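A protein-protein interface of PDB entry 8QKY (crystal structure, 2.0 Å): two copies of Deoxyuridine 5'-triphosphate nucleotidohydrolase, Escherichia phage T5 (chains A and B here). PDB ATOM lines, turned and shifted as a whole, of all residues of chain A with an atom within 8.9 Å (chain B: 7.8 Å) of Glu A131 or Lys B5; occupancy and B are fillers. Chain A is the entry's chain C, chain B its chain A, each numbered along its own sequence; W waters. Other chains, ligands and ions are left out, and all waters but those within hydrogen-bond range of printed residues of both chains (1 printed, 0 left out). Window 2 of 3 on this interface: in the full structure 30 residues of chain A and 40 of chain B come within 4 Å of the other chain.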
ATOM      1  N   PHE A 126      12.554  25.854  13.672  1.00  0.00           N
ATOM      2  CA  PHE A 126      11.703  25.001  14.478  1.00  0.00           C
ATOM      3  C   PHE A 126      10.598  25.846  15.086  1.00  0.00           C
ATOM      4  O   PHE A 126      10.659  27.075  15.099  1.00  0.00           O
ATOM      5  CB  PHE A 126      12.484  24.299  15.594  1.00  0.00           C
ATOM      6  CG  PHE A 126      12.983  25.236  16.648  1.00  0.00           C
ATOM      7  CD1 PHE A 126      12.169  25.620  17.709  1.00  0.00           C
ATOM      8  CD2 PHE A 126      14.264  25.759  16.566  1.00  0.00           C
ATOM      9  CE1 PHE A 126      12.628  26.504  18.671  1.00  0.00           C
ATOM     10  CE2 PHE A 126      14.731  26.635  17.527  1.00  0.00           C
ATOM     11  CZ  PHE A 126      13.912  27.006  18.582  1.00  0.00           C
ATOM     12  N   LYS A 127       9.604  25.159  15.635  1.00  0.00           N
ATOM     13  CA  LYS A 127       8.505  25.801  16.338  1.00  0.00           C
ATOM     14  C   LYS A 127       8.087  24.875  17.469  1.00  0.00           C
ATOM     15  O   LYS A 127       7.911  23.676  17.247  1.00  0.00           O
ATOM     16  CB  LYS A 127       7.333  26.070  15.383  1.00  0.00           C
ATOM     17  CG  LYS A 127       6.093  26.641  16.043  1.00  0.00           C
ATOM     18  CD  LYS A 127       4.996  26.894  15.021  1.00  0.00           C
ATOM     19  CE  LYS A 127       3.885  27.747  15.621  1.00  0.00           C
ATOM     20  NZ  LYS A 127       2.791  27.999  14.637  1.00  0.00           N
ATOM     21  N   ILE A 128       7.964  25.418  18.676  1.00  0.00           N
ATOM     22  CA  ILE A 128       7.440  24.663  19.811  1.00  0.00           C
ATOM     23  C   ILE A 128       5.924  24.647  19.715  1.00  0.00           C
ATOM     24  O   ILE A 128       5.305  25.695  19.507  1.00  0.00           O
ATOM     25  CB  ILE A 128       7.901  25.284  21.140  1.00  0.00           C
ATOM     26  CG1 ILE A 128       9.393  25.625  21.085  1.00  0.00           C
ATOM     27  CG2 ILE A 128       7.547  24.372  22.317  1.00  0.00           C
ATOM     28  CD1 ILE A 128      10.289  24.427  21.010  1.00  0.00           C
ATOM     29  N   VAL A 129       5.322  23.463  19.867  1.00  0.00           N
ATOM     30  CA  VAL A 129       3.882  23.301  19.732  1.00  0.00           C
ATOM     31  C   VAL A 129       3.392  22.496  20.924  1.00  0.00           C
ATOM     32  O   VAL A 129       4.166  21.822  21.606  1.00  0.00           O
ATOM     33  CB  VAL A 129       3.478  22.593  18.413  1.00  0.00           C
ATOM     34  CG1 VAL A 129       3.750  23.493  17.217  1.00  0.00           C
ATOM     35  CG2 VAL A 129       4.191  21.254  18.273  1.00  0.00           C
ATOM     36  N   ASP A 130       2.081  22.568  21.167  1.00  0.00           N
ATOM     37  CA  ASP A 130       1.482  21.792  22.248  1.00  0.00           C
ATOM     38  C   ASP A 130       1.182  20.360  21.830  1.00  0.00           C
ATOM     39  O   ASP A 130       1.170  19.464  22.680  1.00  0.00           O
ATOM     40  CB  ASP A 130       0.194  22.463  22.733  1.00  0.00           C
ATOM     41  CG  ASP A 130       0.458  23.686  23.582  1.00  0.00           C
ATOM     42  OD1 ASP A 130       1.025  23.533  24.688  1.00  0.00           O
ATOM     43  OD2 ASP A 130       0.108  24.805  23.140  1.00  0.00           O
ATOM     44  N   GLU A 131       0.903  20.129  20.548  1.00  0.00           N
ATOM     45  CA  GLU A 131       0.679  18.784  20.039  1.00  0.00           C
ATOM     46  C   GLU A 131       1.227  18.693  18.625  1.00  0.00           C
ATOM     47  O   GLU A 131       1.227  19.674  17.876  1.00  0.00           O
ATOM     48  CB  GLU A 131      -0.810  18.375  20.046  1.00  0.00           C
ATOM     49  CG  GLU A 131      -1.535  18.589  21.367  1.00  0.00           C
ATOM     50  CD  GLU A 131      -1.161  17.538  22.409  1.00  0.00           C
ATOM     51  OE1 GLU A 131      -1.377  17.787  23.620  1.00  0.00           O
ATOM     52  OE2 GLU A 131      -0.630  16.471  22.019  1.00  0.00           O
ATOM     53  N   LEU A 132       1.707  17.508  18.275  1.00  0.00           N
ATOM     54  CA  LEU A 132       2.183  17.228  16.931  1.00  0.00           C
ATOM     55  C   LEU A 132       1.076  16.533  16.148  1.00  0.00           C
ATOM     56  O   LEU A 132       0.155  15.948  16.723  1.00  0.00           O
ATOM     57  CB  LEU A 132       3.440  16.350  16.968  1.00  0.00           C
ATOM     58  CG  LEU A 132       4.548  16.726  17.960  1.00  0.00           C
ATOM     59  CD1 LEU A 132       5.496  15.559  18.173  1.00  0.00           C
ATOM     60  CD2 LEU A 132       5.293  17.939  17.457  1.00  0.00           C
ATOM     61  N   GLU A 133       1.190  16.578  14.822  1.00  0.00           N
ATOM     62  CA  GLU A 133       0.204  15.923  13.967  1.00  0.00           C
ATOM     63  C   GLU A 133       0.393  14.408  14.007  1.00  0.00           C
ATOM     64  O   GLU A 133       1.506  13.906  13.831  1.00  0.00           O
ATOM     65  CB  GLU A 133       0.322  16.441  12.533  1.00  0.00           C
ATOM     66  CG  GLU A 133       0.089  17.944  12.380  1.00  0.00           C
ATOM     67  CD  GLU A 133      -1.317  18.376  12.769  1.00  0.00           C
ATOM     68  OE1 GLU A 133      -2.275  17.628  12.474  1.00  0.00           O
ATOM     69  OE2 GLU A 133      -1.462  19.468  13.360  1.00  0.00           O
ATOM     70  N   GLU A 134      -0.703  13.682  14.225  1.00  0.00           N
ATOM     71  CA  GLU A 134      -0.649  12.249  14.481  1.00  0.00           C
ATOM     72  C   GLU A 134      -0.318  11.454  13.221  1.00  0.00           C
ATOM     73  O   GLU A 134      -0.564  11.893  12.092  1.00  0.00           O
ATOM     74  CB  GLU A 134      -1.981  11.780  15.064  1.00  0.00           C
ATOM     75  CG  GLU A 134      -2.656  12.856  15.905  1.00  0.00           C
ATOM     76  CD  GLU A 134      -3.629  12.290  16.909  1.00  0.00           C
ATOM     77  OE1 GLU A 134      -3.764  11.051  16.967  1.00  0.00           O
ATOM     78  OE2 GLU A 134      -4.246  13.086  17.649  1.00  0.00           O
ATOM     79  N   ILE B   2      10.783  22.123  11.645  1.00  0.00           N
ATOM     80  CA  ILE B   2      10.669  21.057  12.633  1.00  0.00           C
ATOM     81  C   ILE B   2       9.715  21.522  13.721  1.00  0.00           C
ATOM     82  O   ILE B   2       9.883  22.611  14.282  1.00  0.00           O
ATOM     83  CB  ILE B   2      12.040  20.711  13.233  1.00  0.00           C
ATOM     84  CG1 ILE B   2      12.977  20.110  12.190  1.00  0.00           C
ATOM     85  CG2 ILE B   2      11.892  19.695  14.365  1.00  0.00           C
ATOM     86  CD1 ILE B   2      14.442  20.397  12.529  1.00  0.00           C
ATOM     87  N   LYS B   3       8.728  20.700  14.041  1.00  0.00           N
ATOM     88  CA  LYS B   3       7.825  20.985  15.148  1.00  0.00           C
ATOM     89  C   LYS B   3       8.284  20.205  16.380  1.00  0.00           C
ATOM     90  O   LYS B   3       8.643  19.026  16.285  1.00  0.00           O
ATOM     91  CB  LYS B   3       6.383  20.626  14.765  1.00  0.00           C
ATOM     92  CG  LYS B   3       5.730  21.653  13.823  1.00  0.00           C
ATOM     93  CD  LYS B   3       4.558  21.051  13.072  1.00  0.00           C
ATOM     94  CE  LYS B   3       3.361  21.997  13.047  1.00  0.00           C
ATOM     95  NZ  LYS B   3       2.226  21.530  13.905  1.00  0.00           N
ATOM     96  N   ILE B   4       8.302  20.870  17.536  1.00  0.00           N
ATOM     97  CA  ILE B   4       8.848  20.284  18.755  1.00  0.00           C
ATOM     98  C   ILE B   4       7.814  20.369  19.876  1.00  0.00           C
ATOM     99  O   ILE B   4       7.270  21.445  20.148  1.00  0.00           O
ATOM    100  CB  ILE B   4      10.150  20.984  19.185  1.00  0.00           C
ATOM    101  CG1 ILE B   4      11.199  20.931  18.070  1.00  0.00           C
ATOM    102  CG2 ILE B   4      10.672  20.365  20.448  1.00  0.00           C
ATOM    103  CD1 ILE B   4      12.483  21.687  18.423  1.00  0.00           C
ATOM    104  N   LYS B   5       7.581  19.249  20.553  1.00  0.00           N
ATOM    105  CA  LYS B   5       6.695  19.187  21.705  1.00  0.00           C
ATOM    106  C   LYS B   5       7.523  18.786  22.916  1.00  0.00           C
ATOM    107  O   LYS B   5       8.162  17.725  22.913  1.00  0.00           O
ATOM    108  CB  LYS B   5       5.551  18.198  21.457  1.00  0.00           C
ATOM    109  CG  LYS B   5       4.639  17.979  22.651  1.00  0.00           C
ATOM    110  CD  LYS B   5       3.680  16.816  22.398  1.00  0.00           C
ATOM    111  CE  LYS B   5       2.641  16.711  23.505  1.00  0.00           C
ATOM    112  NZ  LYS B   5       2.931  15.550  24.392  1.00  0.00           N
ATOM    113  N   LEU B   6       7.521  19.640  23.937  1.00  0.00           N
ATOM    114  CA  LEU B   6       8.330  19.455  25.137  1.00  0.00           C
ATOM    115  C   LEU B   6       7.459  18.958  26.286  1.00  0.00           C
ATOM    116  O   LEU B   6       6.403  19.533  26.561  1.00  0.00           O
ATOM    117  CB  LEU B   6       9.019  20.767  25.531  1.00  0.00           C
ATOM    118  CG  LEU B   6       9.815  21.505  24.450  1.00  0.00           C
ATOM    119  CD1 LEU B   6      10.401  22.830  24.955  1.00  0.00           C
ATOM    120  CD2 LEU B   6      10.913  20.612  23.922  1.00  0.00           C
ATOM    121  N   THR B   7       7.906  17.896  26.960  1.00  0.00           N
ATOM    122  CA  THR B   7       7.218  17.437  28.166  1.00  0.00           C
ATOM    123  C   THR B   7       7.280  18.478  29.281  1.00  0.00           C
ATOM    124  O   THR B   7       6.352  18.586  30.092  1.00  0.00           O
ATOM    125  CB  THR B   7       7.841  16.120  28.628  1.00  0.00           C
ATOM    126  OG1 THR B   7       7.825  15.191  27.543  1.00  0.00           O
ATOM    127  CG2 THR B   7       7.088  15.528  29.811  1.00  0.00           C
ATOM    128  N   HIS B   8       8.365  19.238  29.342  1.00  0.00           N
ATOM    129  CA  HIS B   8       8.586  20.296  30.310  1.00  0.00           C
ATOM    130  C   HIS B   8       9.380  21.365  29.581  1.00  0.00           C
ATOM    131  O   HIS B   8      10.177  21.030  28.700  1.00  0.00           O
ATOM    132  CB  HIS B   8       9.350  19.779  31.542  1.00  0.00           C
ATOM    133  CG  HIS B   8       9.562  20.810  32.608  1.00  0.00           C
ATOM    134  ND1 HIS B   8      10.522  21.796  32.515  1.00  0.00           N
ATOM    135  CD2 HIS B   8       8.932  21.012  33.791  1.00  0.00           C
ATOM    136  CE1 HIS B   8      10.478  22.555  33.596  1.00  0.00           C
ATOM    137  NE2 HIS B   8       9.520  22.102  34.385  1.00  0.00           N
ATOM    138  N   CYS B  11      13.170  21.018  29.022  1.00  0.00           N
ATOM    139  CA  CYS B  11      13.632  20.017  28.068  1.00  0.00           C
ATOM    140  C   CYS B  11      14.089  20.610  26.742  1.00  0.00           C
ATOM    141  O   CYS B  11      14.647  19.875  25.915  1.00  0.00           O
ATOM    142  CB  CYS B  11      12.524  19.009  27.791  1.00  0.00           C
ATOM    143  SG  CYS B  11      11.964  18.113  29.232  1.00  0.00           S
ATOM    144  N   PRO B  13      15.791  21.560  23.633  1.00  0.00           N
ATOM    145  CA  PRO B  13      17.163  21.275  23.192  1.00  0.00           C
ATOM    146  C   PRO B  13      18.003  22.543  23.100  1.00  0.00           C
ATOM    147  O   PRO B  13      17.511  23.617  22.745  1.00  0.00           O
ATOM    148  CB  PRO B  13      16.970  20.631  21.814  1.00  0.00           C
ATOM    149  CG  PRO B  13      15.567  20.029  21.873  1.00  0.00           C
ATOM    150  CD  PRO B  13      14.779  21.022  22.696  1.00  0.00           C
ATOM    151  N   THR B  50      14.323  12.189  26.748  1.00  0.00           N
ATOM    152  CA  THR B  50      14.704  13.575  26.498  1.00  0.00           C
ATOM    153  C   THR B  50      13.575  14.551  26.798  1.00  0.00           C
ATOM    154  O   THR B  50      13.828  15.756  26.893  1.00  0.00           O
ATOM    155  CB  THR B  50      15.133  13.787  25.042  1.00  0.00           C
ATOM    156  OG1 THR B  50      14.022  13.529  24.184  1.00  0.00           O
ATOM    157  CG2 THR B  50      16.290  12.877  24.662  1.00  0.00           C
ATOM    158  N   GLY B  51      12.343  14.062  26.930  1.00  0.00           N
ATOM    159  CA  GLY B  51      11.194  14.944  26.990  1.00  0.00           C
ATOM    160  C   GLY B  51      10.912  15.696  25.706  1.00  0.00           C
ATOM    161  O   GLY B  51      10.178  16.690  25.719  1.00  0.00           O
ATOM    162  N   VAL B  52      11.482  15.257  24.590  1.00  0.00           N
ATOM    163  CA  VAL B  52      11.392  15.980  23.331  1.00  0.00           C
ATOM    164  C   VAL B  52      10.769  15.046  22.305  1.00  0.00           C
ATOM    165  O   VAL B  52      11.329  13.983  22.003  1.00  0.00           O
ATOM    166  CB  VAL B  52      12.771  16.473  22.858  1.00  0.00           C
ATOM    167  CG1 VAL B  52      12.699  16.990  21.417  1.00  0.00           C
ATOM    168  CG2 VAL B  52      13.332  17.537  23.817  1.00  0.00           C
ATOM    169  N   ALA B  53       9.609  15.432  21.784  1.00  0.00           N
ATOM    170  CA  ALA B  53       8.970  14.757  20.663  1.00  0.00           C
ATOM    171  C   ALA B  53       8.998  15.702  19.473  1.00  0.00           C
ATOM    172  O   ALA B  53       8.806  16.911  19.634  1.00  0.00           O
ATOM    173  CB  ALA B  53       7.522  14.371  20.991  1.00  0.00           C
ATOM    174  N   VAL B  54       9.271  15.171  18.284  1.00  0.00           N
ATOM    175  CA  VAL B  54       9.468  16.036  17.131  1.00  0.00           C
ATOM    176  C   VAL B  54       8.604  15.558  15.985  1.00  0.00           C
ATOM    177  O   VAL B  54       8.258  14.379  15.880  1.00  0.00           O
ATOM    178  CB  VAL B  54      10.944  16.110  16.678  1.00  0.00           C
ATOM    179  CG1 VAL B  54      11.820  16.664  17.802  1.00  0.00           C
ATOM    180  CG2 VAL B  54      11.433  14.742  16.239  1.00  0.00           C
ATOM    181  N   GLU B  55       8.251  16.495  15.133  1.00  0.00           N
ATOM    182  CA  GLU B  55       7.630  16.218  13.849  1.00  0.00           C
ATOM    183  C   GLU B  55       8.662  16.661  12.823  1.00  0.00           C
ATOM    184  O   GLU B  55       8.829  17.857  12.563  1.00  0.00           O
ATOM    185  CB  GLU B  55       6.302  16.960  13.723  1.00  0.00           C
ATOM    186  CG  GLU B  55       5.575  16.763  12.414  1.00  0.00           C
ATOM    187  CD  GLU B  55       4.249  17.530  12.364  1.00  0.00           C
ATOM    188  OE1 GLU B  55       3.846  17.934  11.253  1.00  0.00           O
ATOM    189  OE2 GLU B  55       3.599  17.712  13.428  1.00  0.00           O
ATOM    190  N   ARG B  89       6.362   9.941  16.701  1.00  0.00           N
ATOM    191  CA  ARG B  89       5.741  10.995  17.483  1.00  0.00           C
ATOM    192  C   ARG B  89       5.905  10.815  18.985  1.00  0.00           C
ATOM    193  O   ARG B  89       5.391  11.641  19.747  1.00  0.00           O
ATOM    194  CB  ARG B  89       4.249  11.108  17.127  1.00  0.00           C
ATOM    195  CG  ARG B  89       3.995  11.448  15.658  1.00  0.00           C
ATOM    196  CD  ARG B  89       4.306  12.913  15.351  1.00  0.00           C
ATOM    197  NE  ARG B  89       4.146  13.194  13.930  1.00  0.00           N
ATOM    198  CZ  ARG B  89       5.121  13.125  13.035  1.00  0.00           C
ATOM    199  NH1 ARG B  89       6.366  12.842  13.390  1.00  0.00           N
ATOM    200  NH2 ARG B  89       4.843  13.340  11.751  1.00  0.00           N
ATOM    201  N   GLY B  90       6.590   9.773  19.439  1.00  0.00           N
ATOM    202  CA  GLY B  90       6.940   9.668  20.837  1.00  0.00           C
ATOM    203  C   GLY B  90       8.116  10.572  21.162  1.00  0.00           C
ATOM    204  O   GLY B  90       8.663  11.257  20.300  1.00  0.00           O
ATOM    205  N   THR B  91       8.503  10.589  22.437  1.00  0.00           N
ATOM    206  CA  THR B  91       9.671  11.375  22.805  1.00  0.00           C
ATOM    207  C   THR B  91      10.933  10.590  22.483  1.00  0.00           C
ATOM    208  O   THR B  91      10.964   9.358  22.574  1.00  0.00           O
ATOM    209  CB  THR B  91       9.672  11.744  24.291  1.00  0.00           C
ATOM    210  OG1 THR B  91       9.719  10.545  25.071  1.00  0.00           O
ATOM    211  CG2 THR B  91       8.434  12.553  24.659  1.00  0.00           C
ATOM    212  N   ILE B  92      11.976  11.316  22.083  1.00  0.00           N
ATOM    213  CA  ILE B  92      13.253  10.680  21.795  1.00  0.00           C
ATOM    214  C   ILE B  92      13.859  10.136  23.079  1.00  0.00           C
ATOM    215  O   ILE B  92      13.847  10.798  24.132  1.00  0.00           O
ATOM    216  CB  ILE B  92      14.206  11.676  21.113  1.00  0.00           C
ATOM    217  CG1 ILE B  92      13.651  12.054  19.736  1.00  0.00           C
ATOM    218  CG2 ILE B  92      15.625  11.091  21.022  1.00  0.00           C
ATOM    219  CD1 ILE B  92      14.168  13.403  19.197  1.00  0.00           C
HETATM  220  O   HOH W   1       5.792  21.893  23.992  1.00  0.00           O
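N of Lys A127 is in hydrogen-bond range of O of Ile B2 (2.9 Å).
O of Lys A127 lies within hydrogen-bond range of N of Ile B4 (2.8 Å).
O of Ile B4 lies within hydrogen-bond range of N of Val A129, 2.8 Å away.
OE2 of Glu B55 lies within hydrogen-bond range of N of Glu A133, 3.0 Å away.
The backbone carbonyl oxygen (O) of Glu A133 lies within hydrogen-bond range of the guanidinium group (NE) of Arg B89 (2.7 Å).
The backbone carbonyl oxygen of Lys B3 lies within hydrogen-bond range of the backbone NH of Glu B55, at 2.8 Å.
The backbone NH (N) of Lys B5 is in hydrogen-bond range of the backbone carbonyl oxygen (O) of Ala B53, at 2.8 Å.
NH1 of Arg B89 lies within hydrogen-bond range of O of Val B54, 3.5 Å away.
Phe A126 touches Ile B2 (CA to O, 3.0 Å).
Phe A126 touches Ile B4.
Lys A127 touches Lys B3.
Lys B5 touches Val A129.
Lys B5 touches Glu A131 (CE to OE2, 3.6 Å).
Leu A132 touches Lys B3.
Lys B5 touches Leu A132.
Leu A132 touches Val B54 (CD1 to O, 3.8 Å).
Leu A132 touches Glu B55.
Leu A132 touches Arg B89 (CB to CD, 3.9 Å).
Of the printed residues of chain B, Val A129 touches Ile B4 (2.8 Å) and Lys B5 (3.7 Å).
Printed residues of chain B within 4 Å of Asp A130: Lys B5.
Printed residues of chain B within 4 Å of Glu A131: Lys B5 (3.6 Å).
Printed residues of chain B within 4 Å of Glu A133: Glu B55 and Arg B89.
Printed residues of chain A within 4 Å of Ala B53: Leu A132.
Ile B92 touches none of the printed residues of chain A.
Of the 19 printed residues of chain B, 8 touch a printed residue of chain A.
Of the 9 printed residues of chain A, 8 touch a printed residue of chain B.
Printed residues of chain A that touch a printed residue of chain B: Phe A126, Lys A127, Ile A128, Val A129, Asp A130, Glu A131, Leu A132 and Glu A133.
Hydrophobic or aromatic side chains of chain A within 4 Å of the printed part of chain B: Phe A126, Ile A128, Val A129 and Leu A132.
Among the printed residues, 18 pairs touch across the chains.
Among the printed residues, no Asp or Glu carboxylate lies within 4 Å of a Lys or Arg side-chain nitrogen of the other chain.
No position is printed for both chains.
Of the 18 pairs that touch across the chains among the printed residues, none has its exchanged pair printed and touching as well.
Water W1 bridges N of Leu B6 and O of Val A129.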
